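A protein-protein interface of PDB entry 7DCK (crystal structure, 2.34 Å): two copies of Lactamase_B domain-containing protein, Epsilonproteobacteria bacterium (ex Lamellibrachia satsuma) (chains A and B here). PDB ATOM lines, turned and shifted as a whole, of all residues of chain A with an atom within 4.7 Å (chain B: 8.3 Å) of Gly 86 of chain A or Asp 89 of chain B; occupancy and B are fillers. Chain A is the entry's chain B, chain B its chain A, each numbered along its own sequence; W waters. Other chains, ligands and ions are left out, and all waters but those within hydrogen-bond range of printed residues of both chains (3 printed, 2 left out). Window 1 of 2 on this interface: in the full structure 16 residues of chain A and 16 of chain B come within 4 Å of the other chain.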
ATOM      1  N   THR A  51      16.605  18.193  -7.537  1.00  0.00           N
ATOM      2  CA  THR A  51      16.587  18.752  -8.883  1.00  0.00           C
ATOM      3  C   THR A  51      17.059  20.203  -8.944  1.00  0.00           C
ATOM      4  O   THR A  51      16.904  20.844  -9.994  1.00  0.00           O
ATOM      5  CB  THR A  51      15.169  18.670  -9.483  1.00  0.00           C
ATOM      6  OG1 THR A  51      14.287  19.528  -8.745  1.00  0.00           O
ATOM      7  CG2 THR A  51      14.623  17.235  -9.443  1.00  0.00           C
ATOM      8  N   GLY A  52      17.621  20.747  -7.865  1.00  0.00           N
ATOM      9  CA  GLY A  52      18.023  22.137  -7.870  1.00  0.00           C
ATOM     10  C   GLY A  52      16.835  23.098  -7.844  1.00  0.00           C
ATOM     11  O   GLY A  52      15.676  22.725  -7.614  1.00  0.00           O
ATOM     12  N   SER A  53      17.152  24.370  -8.091  1.00  0.00           N
ATOM     13  CA  SER A  53      16.140  25.417  -8.148  1.00  0.00           C
ATOM     14  C   SER A  53      15.720  25.767  -9.564  1.00  0.00           C
ATOM     15  O   SER A  53      14.760  26.524  -9.733  1.00  0.00           O
ATOM     16  CB  SER A  53      16.646  26.690  -7.463  1.00  0.00           C
ATOM     17  OG  SER A  53      17.870  27.127  -8.033  1.00  0.00           O
ATOM     18  N   ASN A  54      16.414  25.249 -10.575  1.00  0.00           N
ATOM     19  CA  ASN A  54      16.227  25.690 -11.958  1.00  0.00           C
ATOM     20  C   ASN A  54      16.465  24.492 -12.867  1.00  0.00           C
ATOM     21  O   ASN A  54      17.612  24.066 -13.049  1.00  0.00           O
ATOM     22  CB  ASN A  54      17.176  26.848 -12.288  1.00  0.00           C
ATOM     23  CG  ASN A  54      16.979  27.397 -13.692  1.00  0.00           C
ATOM     24  OD1 ASN A  54      16.878  26.639 -14.653  1.00  0.00           O
ATOM     25  ND2 ASN A  54      16.927  28.726 -13.816  1.00  0.00           N
ATOM     26  N   GLY A  55      15.389  23.955 -13.442  1.00  0.00           N
ATOM     27  CA  GLY A  55      15.508  22.773 -14.278  1.00  0.00           C
ATOM     28  C   GLY A  55      16.187  23.015 -15.610  1.00  0.00           C
ATOM     29  O   GLY A  55      16.737  22.073 -16.192  1.00  0.00           O
ATOM     30  N   ARG A  56      16.150  24.250 -16.115  1.00  0.00           N
ATOM     31  CA  ARG A  56      16.831  24.537 -17.373  1.00  0.00           C
ATOM     32  C   ARG A  56      18.344  24.499 -17.185  1.00  0.00           C
ATOM     33  O   ARG A  56      19.071  23.926 -18.005  1.00  0.00           O
ATOM     34  CB  ARG A  56      16.383  25.891 -17.927  1.00  0.00           C
ATOM     35  CG  ARG A  56      14.871  26.115 -17.926  1.00  0.00           C
ATOM     36  CD  ARG A  56      14.088  24.906 -18.450  1.00  0.00           C
ATOM     37  NE  ARG A  56      14.328  24.615 -19.863  1.00  0.00           N
ATOM     38  CZ  ARG A  56      14.057  23.446 -20.443  1.00  0.00           C
ATOM     39  NH1 ARG A  56      13.539  22.450 -19.733  1.00  0.00           N
ATOM     40  NH2 ARG A  56      14.303  23.266 -21.733  1.00  0.00           N
ATOM     41  N   TRP A  82      11.885  25.102  -2.623  1.00  0.00           N
ATOM     42  CA  TRP A  82      12.032  25.544  -4.011  1.00  0.00           C
ATOM     43  C   TRP A  82      13.373  25.132  -4.612  1.00  0.00           C
ATOM     44  O   TRP A  82      13.460  24.842  -5.809  1.00  0.00           O
ATOM     45  CB  TRP A  82      11.865  27.069  -4.090  1.00  0.00           C
ATOM     46  CG  TRP A  82      12.904  27.812  -3.298  1.00  0.00           C
ATOM     47  CD1 TRP A  82      12.901  28.033  -1.948  1.00  0.00           C
ATOM     48  CD2 TRP A  82      14.114  28.408  -3.797  1.00  0.00           C
ATOM     49  NE1 TRP A  82      14.027  28.733  -1.578  1.00  0.00           N
ATOM     50  CE2 TRP A  82      14.787  28.975  -2.691  1.00  0.00           C
ATOM     51  CE3 TRP A  82      14.691  28.521  -5.065  1.00  0.00           C
ATOM     52  CZ2 TRP A  82      16.007  29.643  -2.819  1.00  0.00           C
ATOM     53  CZ3 TRP A  82      15.903  29.186  -5.188  1.00  0.00           C
ATOM     54  CH2 TRP A  82      16.547  29.735  -4.073  1.00  0.00           C
ATOM     55  N   HIS A  84      15.104  22.502  -4.268  1.00  0.00           N
ATOM     56  CA  HIS A  84      15.306  21.078  -4.479  1.00  0.00           C
ATOM     57  C   HIS A  84      14.284  20.444  -5.406  1.00  0.00           C
ATOM     58  O   HIS A  84      14.590  19.408  -6.007  1.00  0.00           O
ATOM     59  CB  HIS A  84      15.314  20.339  -3.133  1.00  0.00           C
ATOM     60  CG  HIS A  84      16.413  20.794  -2.224  1.00  0.00           C
ATOM     61  ND1 HIS A  84      17.572  20.072  -2.036  1.00  0.00           N
ATOM     62  CD2 HIS A  84      16.548  21.919  -1.484  1.00  0.00           C
ATOM     63  CE1 HIS A  84      18.365  20.721  -1.202  1.00  0.00           C
ATOM     64  NE2 HIS A  84      17.766  21.845  -0.852  1.00  0.00           N
ATOM     65  N   ILE A  85      13.105  21.041  -5.564  1.00  0.00           N
ATOM     66  CA  ILE A  85      12.097  20.580  -6.509  1.00  0.00           C
ATOM     67  C   ILE A  85      11.959  21.532  -7.691  1.00  0.00           C
ATOM     68  O   ILE A  85      11.081  21.340  -8.541  1.00  0.00           O
ATOM     69  CB  ILE A  85      10.743  20.366  -5.812  1.00  0.00           C
ATOM     70  CG1 ILE A  85      10.054  21.711  -5.548  1.00  0.00           C
ATOM     71  CG2 ILE A  85      10.939  19.620  -4.508  1.00  0.00           C
ATOM     72  CD1 ILE A  85       8.601  21.580  -5.140  1.00  0.00           C
ATOM     73  N   GLY A  86      12.821  22.545  -7.781  1.00  0.00           N
ATOM     74  CA  GLY A  86      12.712  23.546  -8.831  1.00  0.00           C
ATOM     75  C   GLY A  86      13.000  23.048 -10.234  1.00  0.00           C
ATOM     76  O   GLY A  86      12.812  23.811 -11.190  1.00  0.00           O
ATOM     77  N   GLY A  87      13.444  21.802 -10.386  1.00  0.00           N
ATOM     78  CA  GLY A  87      13.741  21.280 -11.703  1.00  0.00           C
ATOM     79  C   GLY A  87      12.923  20.068 -12.099  1.00  0.00           C
ATOM     80  O   GLY A  87      13.174  19.461 -13.144  1.00  0.00           O
ATOM     81  N   VAL A  88      11.931  19.719 -11.277  1.00  0.00           N
ATOM     82  CA  VAL A  88      11.171  18.489 -11.485  1.00  0.00           C
ATOM     83  C   VAL A  88      10.458  18.512 -12.834  1.00  0.00           C
ATOM     84  O   VAL A  88      10.474  17.528 -13.581  1.00  0.00           O
ATOM     85  CB  VAL A  88      10.182  18.271 -10.325  1.00  0.00           C
ATOM     86  CG1 VAL A  88       9.146  17.226 -10.695  1.00  0.00           C
ATOM     87  CG2 VAL A  88      10.919  17.851  -9.068  1.00  0.00           C
ATOM     88  N   ASP A  89       9.820  19.634 -13.169  1.00  0.00           N
ATOM     89  CA  ASP A  89       9.035  19.683 -14.401  1.00  0.00           C
ATOM     90  C   ASP A  89       9.915  19.493 -15.633  1.00  0.00           C
ATOM     91  O   ASP A  89       9.541  18.763 -16.560  1.00  0.00           O
ATOM     92  CB  ASP A  89       8.257  20.998 -14.485  1.00  0.00           C
ATOM     93  CG  ASP A  89       9.140  22.221 -14.298  1.00  0.00           C
ATOM     94  OD1 ASP A  89      10.171  22.131 -13.589  1.00  0.00           O
ATOM     95  OD2 ASP A  89       8.797  23.281 -14.861  1.00  0.00           O
ATOM     96  N   SER A  90      11.090  20.137 -15.662  1.00  0.00           N
ATOM     97  CA  SER A  90      12.001  19.965 -16.792  1.00  0.00           C
ATOM     98  C   SER A  90      12.510  18.532 -16.890  1.00  0.00           C
ATOM     99  O   SER A  90      12.671  17.994 -17.989  1.00  0.00           O
ATOM    100  CB  SER A  90      13.190  20.918 -16.682  1.00  0.00           C
ATOM    101  OG  SER A  90      12.834  22.264 -16.934  1.00  0.00           O
ATOM    102  N   THR B  51       3.238  31.979 -12.530  1.00  0.00           N
ATOM    103  CA  THR B  51       3.758  31.109 -13.578  1.00  0.00           C
ATOM    104  C   THR B  51       3.302  29.658 -13.440  1.00  0.00           C
ATOM    105  O   THR B  51       3.896  28.776 -14.074  1.00  0.00           O
ATOM    106  CB  THR B  51       5.294  31.139 -13.601  1.00  0.00           C
ATOM    107  OG1 THR B  51       5.806  30.620 -12.366  1.00  0.00           O
ATOM    108  CG2 THR B  51       5.805  32.541 -13.806  1.00  0.00           C
ATOM    109  N   SER B  53       2.626  25.841 -11.810  1.00  0.00           N
ATOM    110  CA  SER B  53       3.494  24.869 -11.159  1.00  0.00           C
ATOM    111  C   SER B  53       4.444  24.175 -12.125  1.00  0.00           C
ATOM    112  O   SER B  53       5.404  23.535 -11.677  1.00  0.00           O
ATOM    113  CB  SER B  53       2.653  23.810 -10.440  1.00  0.00           C
ATOM    114  OG  SER B  53       1.830  23.117 -11.360  1.00  0.00           O
ATOM    115  N   ASN B  54       4.211  24.298 -13.429  1.00  0.00           N
ATOM    116  CA  ASN B  54       4.959  23.560 -14.441  1.00  0.00           C
ATOM    117  C   ASN B  54       5.253  24.514 -15.591  1.00  0.00           C
ATOM    118  O   ASN B  54       4.349  24.860 -16.360  1.00  0.00           O
ATOM    119  CB  ASN B  54       4.162  22.344 -14.916  1.00  0.00           C
ATOM    120  CG  ASN B  54       4.986  21.392 -15.759  1.00  0.00           C
ATOM    121  OD1 ASN B  54       5.617  21.796 -16.735  1.00  0.00           O
ATOM    122  ND2 ASN B  54       4.968  20.112 -15.395  1.00  0.00           N
ATOM    123  N   GLY B  55       6.516  24.936 -15.710  1.00  0.00           N
ATOM    124  CA  GLY B  55       6.878  25.901 -16.736  1.00  0.00           C
ATOM    125  C   GLY B  55       6.835  25.347 -18.146  1.00  0.00           C
ATOM    126  O   GLY B  55       6.612  26.098 -19.103  1.00  0.00           O
ATOM    127  N   ARG B  56       7.062  24.040 -18.305  1.00  0.00           N
ATOM    128  CA  ARG B  56       6.950  23.438 -19.630  1.00  0.00           C
ATOM    129  C   ARG B  56       5.505  23.461 -20.112  1.00  0.00           C
ATOM    130  O   ARG B  56       5.225  23.858 -21.249  1.00  0.00           O
ATOM    131  CB  ARG B  56       7.499  22.012 -19.619  1.00  0.00           C
ATOM    132  CG  ARG B  56       8.819  21.839 -18.876  1.00  0.00           C
ATOM    133  CD  ARG B  56       9.844  22.901 -19.263  1.00  0.00           C
ATOM    134  NE  ARG B  56      10.178  22.883 -20.686  1.00  0.00           N
ATOM    135  CZ  ARG B  56      10.731  23.907 -21.331  1.00  0.00           C
ATOM    136  NH1 ARG B  56      11.005  25.032 -20.683  1.00  0.00           N
ATOM    137  NH2 ARG B  56      11.004  23.810 -22.624  1.00  0.00           N
ATOM    138  N   LEU B  58       3.266  25.502 -18.991  1.00  0.00           N
ATOM    139  CA  LEU B  58       2.922  26.916 -19.119  1.00  0.00           C
ATOM    140  C   LEU B  58       3.299  27.451 -20.498  1.00  0.00           C
ATOM    141  O   LEU B  58       2.495  28.127 -21.154  1.00  0.00           O
ATOM    142  CB  LEU B  58       3.608  27.732 -18.018  1.00  0.00           C
ATOM    143  CG  LEU B  58       3.431  29.251 -18.116  1.00  0.00           C
ATOM    144  CD1 LEU B  58       1.983  29.641 -17.903  1.00  0.00           C
ATOM    145  CD2 LEU B  58       4.316  29.966 -17.115  1.00  0.00           C
ATOM    146  N   LEU B  59       4.522  27.156 -20.957  1.00  0.00           N
ATOM    147  CA  LEU B  59       4.941  27.615 -22.280  1.00  0.00           C
ATOM    148  C   LEU B  59       4.099  26.982 -23.384  1.00  0.00           C
ATOM    149  O   LEU B  59       3.747  27.651 -24.364  1.00  0.00           O
ATOM    150  CB  LEU B  59       6.420  27.312 -22.505  1.00  0.00           C
ATOM    151  CG  LEU B  59       7.448  28.061 -21.653  1.00  0.00           C
ATOM    152  CD1 LEU B  59       8.858  27.698 -22.095  1.00  0.00           C
ATOM    153  CD2 LEU B  59       7.236  29.568 -21.713  1.00  0.00           C
ATOM    154  N   LEU B  69       5.068  35.334 -25.256  1.00  0.00           N
ATOM    155  CA  LEU B  69       5.720  35.691 -24.002  1.00  0.00           C
ATOM    156  C   LEU B  69       6.671  36.871 -24.162  1.00  0.00           C
ATOM    157  O   LEU B  69       6.814  37.686 -23.243  1.00  0.00           O
ATOM    158  CB  LEU B  69       6.471  34.469 -23.472  1.00  0.00           C
ATOM    159  CG  LEU B  69       7.290  34.586 -22.192  1.00  0.00           C
ATOM    160  CD1 LEU B  69       6.421  35.121 -21.097  1.00  0.00           C
ATOM    161  CD2 LEU B  69       7.811  33.222 -21.815  1.00  0.00           C
ATOM    162  N   LEU B  75       7.301  40.434 -14.952  1.00  0.00           N
ATOM    163  CA  LEU B  75       6.772  39.227 -14.338  1.00  0.00           C
ATOM    164  C   LEU B  75       6.469  39.535 -12.879  1.00  0.00           C
ATOM    165  O   LEU B  75       7.339  40.020 -12.149  1.00  0.00           O
ATOM    166  CB  LEU B  75       7.762  38.058 -14.463  1.00  0.00           C
ATOM    167  CG  LEU B  75       7.601  36.849 -13.534  1.00  0.00           C
ATOM    168  CD1 LEU B  75       6.257  36.167 -13.735  1.00  0.00           C
ATOM    169  CD2 LEU B  75       8.732  35.855 -13.753  1.00  0.00           C
ATOM    170  N   TRP B  82       4.895  26.715  -4.522  1.00  0.00           N
ATOM    171  CA  TRP B  82       5.382  25.960  -5.677  1.00  0.00           C
ATOM    172  C   TRP B  82       4.480  26.098  -6.897  1.00  0.00           C
ATOM    173  O   TRP B  82       4.966  26.114  -8.033  1.00  0.00           O
ATOM    174  CB  TRP B  82       5.505  24.483  -5.298  1.00  0.00           C
ATOM    175  CG  TRP B  82       4.188  23.918  -4.852  1.00  0.00           C
ATOM    176  CD1 TRP B  82       3.627  24.024  -3.609  1.00  0.00           C
ATOM    177  CD2 TRP B  82       3.241  23.201  -5.658  1.00  0.00           C
ATOM    178  NE1 TRP B  82       2.401  23.400  -3.588  1.00  0.00           N
ATOM    179  CE2 TRP B  82       2.139  22.889  -4.833  1.00  0.00           C
ATOM    180  CE3 TRP B  82       3.222  22.786  -6.994  1.00  0.00           C
ATOM    181  CZ2 TRP B  82       1.029  22.178  -5.300  1.00  0.00           C
ATOM    182  CZ3 TRP B  82       2.114  22.078  -7.459  1.00  0.00           C
ATOM    183  CH2 TRP B  82       1.036  21.782  -6.613  1.00  0.00           C
ATOM    184  N   ILE B  85       5.302  29.760  -8.611  1.00  0.00           N
ATOM    185  CA  ILE B  85       6.650  30.047  -9.085  1.00  0.00           C
ATOM    186  C   ILE B  85       7.249  28.861  -9.830  1.00  0.00           C
ATOM    187  O   ILE B  85       8.424  28.906 -10.215  1.00  0.00           O
ATOM    188  CB  ILE B  85       7.564  30.481  -7.928  1.00  0.00           C
ATOM    189  CG1 ILE B  85       7.816  29.308  -6.972  1.00  0.00           C
ATOM    190  CG2 ILE B  85       6.952  31.652  -7.183  1.00  0.00           C
ATOM    191  CD1 ILE B  85       8.950  29.542  -5.997  1.00  0.00           C
ATOM    192  N   GLY B  86       6.467  27.803 -10.055  1.00  0.00           N
ATOM    193  CA  GLY B  86       6.976  26.596 -10.684  1.00  0.00           C
ATOM    194  C   GLY B  86       7.424  26.772 -12.121  1.00  0.00           C
ATOM    195  O   GLY B  86       8.174  25.930 -12.629  1.00  0.00           O
ATOM    196  N   GLY B  87       6.984  27.835 -12.787  1.00  0.00           N
ATOM    197  CA  GLY B  87       7.353  28.092 -14.163  1.00  0.00           C
ATOM    198  C   GLY B  87       8.331  29.223 -14.385  1.00  0.00           C
ATOM    199  O   GLY B  87       8.589  29.575 -15.544  1.00  0.00           O
ATOM    200  N   VAL B  88       8.903  29.791 -13.320  1.00  0.00           N
ATOM    201  CA  VAL B  88       9.733  30.985 -13.458  1.00  0.00           C
ATOM    202  C   VAL B  88      10.964  30.696 -14.309  1.00  0.00           C
ATOM    203  O   VAL B  88      11.301  31.466 -15.216  1.00  0.00           O
ATOM    204  CB  VAL B  88      10.122  31.533 -12.073  1.00  0.00           C
ATOM    205  CG1 VAL B  88      11.201  32.607 -12.210  1.00  0.00           C
ATOM    206  CG2 VAL B  88       8.891  32.088 -11.370  1.00  0.00           C
ATOM    207  N   ASP B  89      11.654  29.585 -14.035  1.00  0.00           N
ATOM    208  CA  ASP B  89      12.898  29.310 -14.751  1.00  0.00           C
ATOM    209  C   ASP B  89      12.655  29.118 -16.246  1.00  0.00           C
ATOM    210  O   ASP B  89      13.449  29.584 -17.075  1.00  0.00           O
ATOM    211  CB  ASP B  89      13.609  28.091 -14.153  1.00  0.00           C
ATOM    212  CG  ASP B  89      12.745  26.840 -14.150  1.00  0.00           C
ATOM    213  OD1 ASP B  89      11.501  26.957 -14.186  1.00  0.00           O
ATOM    214  OD2 ASP B  89      13.320  25.733 -14.107  1.00  0.00           O
ATOM    215  N   SER B  90      11.556  28.452 -16.615  1.00  0.00           N
ATOM    216  CA  SER B  90      11.250  28.273 -18.033  1.00  0.00           C
ATOM    217  C   SER B  90      10.949  29.603 -18.716  1.00  0.00           C
ATOM    218  O   SER B  90      11.336  29.814 -19.872  1.00  0.00           O
ATOM    219  CB  SER B  90      10.075  27.313 -18.197  1.00  0.00           C
ATOM    220  OG  SER B  90      10.494  25.973 -18.013  1.00  0.00           O
ATOM    221  N   VAL B  91      10.260  30.511 -18.023  1.00  0.00           N
ATOM    222  CA  VAL B  91       9.913  31.797 -18.624  1.00  0.00           C
ATOM    223  C   VAL B  91      11.157  32.657 -18.813  1.00  0.00           C
ATOM    224  O   VAL B  91      11.325  33.314 -19.848  1.00  0.00           O
ATOM    225  CB  VAL B  91       8.854  32.514 -17.765  1.00  0.00           C
ATOM    226  CG1 VAL B  91       8.677  33.940 -18.228  1.00  0.00           C
ATOM    227  CG2 VAL B  91       7.524  31.763 -17.815  1.00  0.00           C
ATOM    228  N   LEU B  92      12.051  32.665 -17.825  1.00  0.00           N
ATOM    229  CA  LEU B  92      13.231  33.520 -17.898  1.00  0.00           C
ATOM    230  C   LEU B  92      14.264  32.994 -18.883  1.00  0.00           C
ATOM    231  O   LEU B  92      15.071  33.774 -19.395  1.00  0.00           O
ATOM    232  CB  LEU B  92      13.849  33.675 -16.510  1.00  0.00           C
ATOM    233  CG  LEU B  92      12.908  34.343 -15.511  1.00  0.00           C
ATOM    234  CD1 LEU B  92      13.592  34.556 -14.181  1.00  0.00           C
ATOM    235  CD2 LEU B  92      12.395  35.661 -16.071  1.00  0.00           C
ATOM    236  N   GLU B  93      14.260  31.690 -19.164  1.00  0.00           N
ATOM    237  CA  GLU B  93      15.175  31.165 -20.171  1.00  0.00           C
ATOM    238  C   GLU B  93      14.833  31.703 -21.557  1.00  0.00           C
ATOM    239  O   GLU B  93      15.725  32.095 -22.316  1.00  0.00           O
ATOM    240  CB  GLU B  93      15.159  29.636 -20.164  1.00  0.00           C
ATOM    241  CG  GLU B  93      16.055  29.015 -21.233  1.00  0.00           C
ATOM    242  CD  GLU B  93      15.827  27.523 -21.401  1.00  0.00           C
ATOM    243  OE1 GLU B  93      16.784  26.814 -21.780  1.00  0.00           O
ATOM    244  OE2 GLU B  93      14.694  27.057 -21.154  1.00  0.00           O
ATOM    245  N   VAL B  94      13.546  31.743 -21.903  1.00  0.00           N
ATOM    246  CA  VAL B  94      13.176  32.214 -23.235  1.00  0.00           C
ATOM    247  C   VAL B  94      13.052  33.735 -23.280  1.00  0.00           C
ATOM    248  O   VAL B  94      13.270  34.340 -24.335  1.00  0.00           O
ATOM    249  CB  VAL B  94      11.879  31.537 -23.717  1.00  0.00           C
ATOM    250  CG1 VAL B  94      12.114  30.058 -23.981  1.00  0.00           C
ATOM    251  CG2 VAL B  94      10.782  31.709 -22.711  1.00  0.00           C
ATOM    252  N   HIS B  95      12.718  34.383 -22.164  1.00  0.00           N
ATOM    253  CA  HIS B  95      12.511  35.834 -22.136  1.00  0.00           C
ATOM    254  C   HIS B  95      13.069  36.419 -20.846  1.00  0.00           C
ATOM    255  O   HIS B  95      12.320  36.802 -19.939  1.00  0.00           O
ATOM    256  CB  HIS B  95      11.028  36.171 -22.301  1.00  0.00           C
ATOM    257  CG  HIS B  95      10.751  37.633 -22.462  1.00  0.00           C
ATOM    258  ND1 HIS B  95      11.595  38.481 -23.144  1.00  0.00           N
ATOM    259  CD2 HIS B  95       9.712  38.395 -22.043  1.00  0.00           C
ATOM    260  CE1 HIS B  95      11.096  39.705 -23.129  1.00  0.00           C
ATOM    261  NE2 HIS B  95       9.954  39.679 -22.468  1.00  0.00           N
ATOM    262  N   PRO B  96      14.400  36.530 -20.738  1.00  0.00           N
ATOM    263  CA  PRO B  96      14.989  37.101 -19.514  1.00  0.00           C
ATOM    264  C   PRO B  96      14.839  38.609 -19.405  1.00  0.00           C
ATOM    265  O   PRO B  96      14.917  39.141 -18.291  1.00  0.00           O
ATOM    266  CB  PRO B  96      16.466  36.705 -19.622  1.00  0.00           C
ATOM    267  CG  PRO B  96      16.711  36.640 -21.094  1.00  0.00           C
ATOM    268  CD  PRO B  96      15.432  36.109 -21.703  1.00  0.00           C
ATOM    269  N   LEU B 110      16.769  33.171  -3.537  1.00  0.00           N
ATOM    270  CA  LEU B 110      16.071  33.174  -4.817  1.00  0.00           C
ATOM    271  C   LEU B 110      16.062  34.569  -5.435  1.00  0.00           C
ATOM    272  O   LEU B 110      16.208  34.714  -6.655  1.00  0.00           O
ATOM    273  CB  LEU B 110      14.645  32.645  -4.638  1.00  0.00           C
ATOM    274  CG  LEU B 110      13.735  32.635  -5.872  1.00  0.00           C
ATOM    275  CD1 LEU B 110      14.424  32.002  -7.081  1.00  0.00           C
ATOM    276  CD2 LEU B 110      12.438  31.913  -5.556  1.00  0.00           C
ATOM    277  N   LEU B 114      17.484  35.631  -9.118  1.00  0.00           N
ATOM    278  CA  LEU B 114      16.670  36.266 -10.148  1.00  0.00           C
ATOM    279  C   LEU B 114      17.265  37.597 -10.593  1.00  0.00           C
ATOM    280  O   LEU B 114      17.126  37.975 -11.763  1.00  0.00           O
ATOM    281  CB  LEU B 114      15.242  36.462  -9.647  1.00  0.00           C
ATOM    282  CG  LEU B 114      14.451  35.185  -9.363  1.00  0.00           C
ATOM    283  CD1 LEU B 114      13.102  35.513  -8.737  1.00  0.00           C
ATOM    284  CD2 LEU B 114      14.278  34.377 -10.638  1.00  0.00           C
ATOM    285  N   GLN B 117      19.833  37.146 -13.379  1.00  0.00           N
ATOM    286  CA  GLN B 117      19.338  36.630 -14.649  1.00  0.00           C
ATOM    287  C   GLN B 117      18.381  37.566 -15.379  1.00  0.00           C
ATOM    288  O   GLN B 117      18.081  37.312 -16.551  1.00  0.00           O
ATOM    289  CB  GLN B 117      18.634  35.280 -14.449  1.00  0.00           C
ATOM    290  CG  GLN B 117      19.422  34.247 -13.654  1.00  0.00           C
ATOM    291  CD  GLN B 117      18.633  32.969 -13.425  1.00  0.00           C
ATOM    292  OE1 GLN B 117      18.816  32.287 -12.419  1.00  0.00           O
ATOM    293  NE2 GLN B 117      17.753  32.636 -14.368  1.00  0.00           N
HETATM  294  O   HOH W   1       6.767  18.268 -17.171  1.00  0.00           O
HETATM  295  O   HOH W   2      16.184  29.901 -16.319  1.00  0.00           O
HETATM  296  O   HOH W   3       9.296  23.940 -11.689  1.00  0.00           O
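The guanidinium group (NE) of Arg 56 of chain A lies close to the guanidinium group (NH1) of Arg 56 of chain B (3.4 Å).
N of Gly 55 of chain B lies within hydrogen-bond range of OD2 of Asp 89 of chain A (2.9 Å).
The side-chain carboxylate of Glu 93 of chain B lies within salt-bridge range of the guanidinium group of Arg 56 of chain A (2.8 Å).
The side-chain carboxylate (OD2) of Asp 89 of chain B is in hydrogen-bond range of the backbone NH (N) of Gly 55 of chain A (2.8 Å).
NH1 of Arg 56 of chain A lies within hydrogen-bond range of OG of Ser 90 of chain A (2.9 Å).
OG1 of Thr 51 of chain A sits at hydrogen-bond distance from N of Gly 86 of chain A, at 3.5 Å.
N of Gly 55 of chain A is in hydrogen-bond range of O of Gly 86 of chain A, at 3.4 Å.
The backbone carbonyl oxygen (O) of Gly 52 of chain A is in hydrogen-bond range of the backbone NH (N) of Gly 86 of chain A, at 2.9 Å.
OD1 of Asn 54 of chain B is in hydrogen-bond range of N of Arg 56 of chain B.
The side-chain amide oxygen (OD1) of Asn 54 of chain A sits at hydrogen-bond distance from the backbone NH (N) of Arg 56 of chain A, at 2.9 Å.
CB of Asp 89 of chain B touches ND2 of Asn 54 of chain A, 3.4 Å away.
Asp 89 of chain B touches Arg 56 of chain A.
Arg 56 of chain A touches Ser 90 of chain B.
Leu 110 of chain B touches Trp 82 of chain A.
Gly 86 of chain A touches Asp 89 of chain B (O to OD2, 3.5 Å).
Asp 89 of chain A touches Asn 54 of chain B (CB to ND2, 3.5 Å).
Asp 89 of chain A touches Arg 56 of chain B (O to CG, 3.9 Å).
Asp 89 of chain A touches Gly 86 of chain B.
Ser 90 of chain A touches Arg 56 of chain B.
Gly 86 of chain A touches just one residue of chain B: Asp 89.
Asp 89 of chain B touches four residues of chain A.
Of the printed residues of chain B, Asn 54 of chain A touches Asp 89.
Printed residues of chain A within 4 Å of Gly 86 of chain B: Asp 89 (3.5 Å).
The nearest residue of chain A that does not touch Asp 89 of chain B is Ser 90 of chain A (4.5 Å).
The nearest printed residue of chain A that does not touch Leu 110 of chain B is Ser 53 of chain A (5.8 Å).
Along chain B the printed residues that touch a printed residue of chain A span positions 54 to 110.
Of the 14 printed residues of chain A, 7 touch a printed residue of chain B.
Hydrophobic or aromatic side chains of chain A within 4 Å of the printed part of chain B: Trp 82.
Among the printed residues, Asp or Glu carboxylates within 4 Å of a Lys or Arg side-chain nitrogen of the other chain: Arg 56 of chain A with Glu 93 of chain B (2.8 Å).
Asn 54 of chain A touches Asp 89 of chain B, and with the chains exchanged Asp 89 of chain A touches Asn 54 of chain B.
Gly 55 of chain A touches Asp 89 of chain B, and with the chains exchanged Asp 89 of chain A touches Gly 55 of chain B.
Arg 56 of chain A touches Ser 90 of chain B, and with the chains exchanged Ser 90 of chain A touches Arg 56 of chain B.
Gly 86 of chain A touches Asp 89 of chain B, and with the chains exchanged Asp 89 of chain A touches Gly 86 of chain B.
12 positions are printed for both chains.
Of the 13 pairs that touch across the chains among the printed residues, 11 have their exchanged pair printed and touching as well.
Water W3 bridges the backbone carbonyl oxygen (O) of Gly 86 of chain B (2.5 Å) and the side-chain carboxylate (OD1) of Asp 89 of chain A (2.8 Å).
Water W2 bridges O of Asp 89 of chain B (2.9 Å) and ND2 of Asn 54 of chain A (2.9 Å).
Water W1 lies within hydrogen-bond range of the backbone carbonyl oxygen of Asp 89 of chain A (2.9 Å) and the side-chain amide nitrogen of Asn 54 of chain B (3.1 Å).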
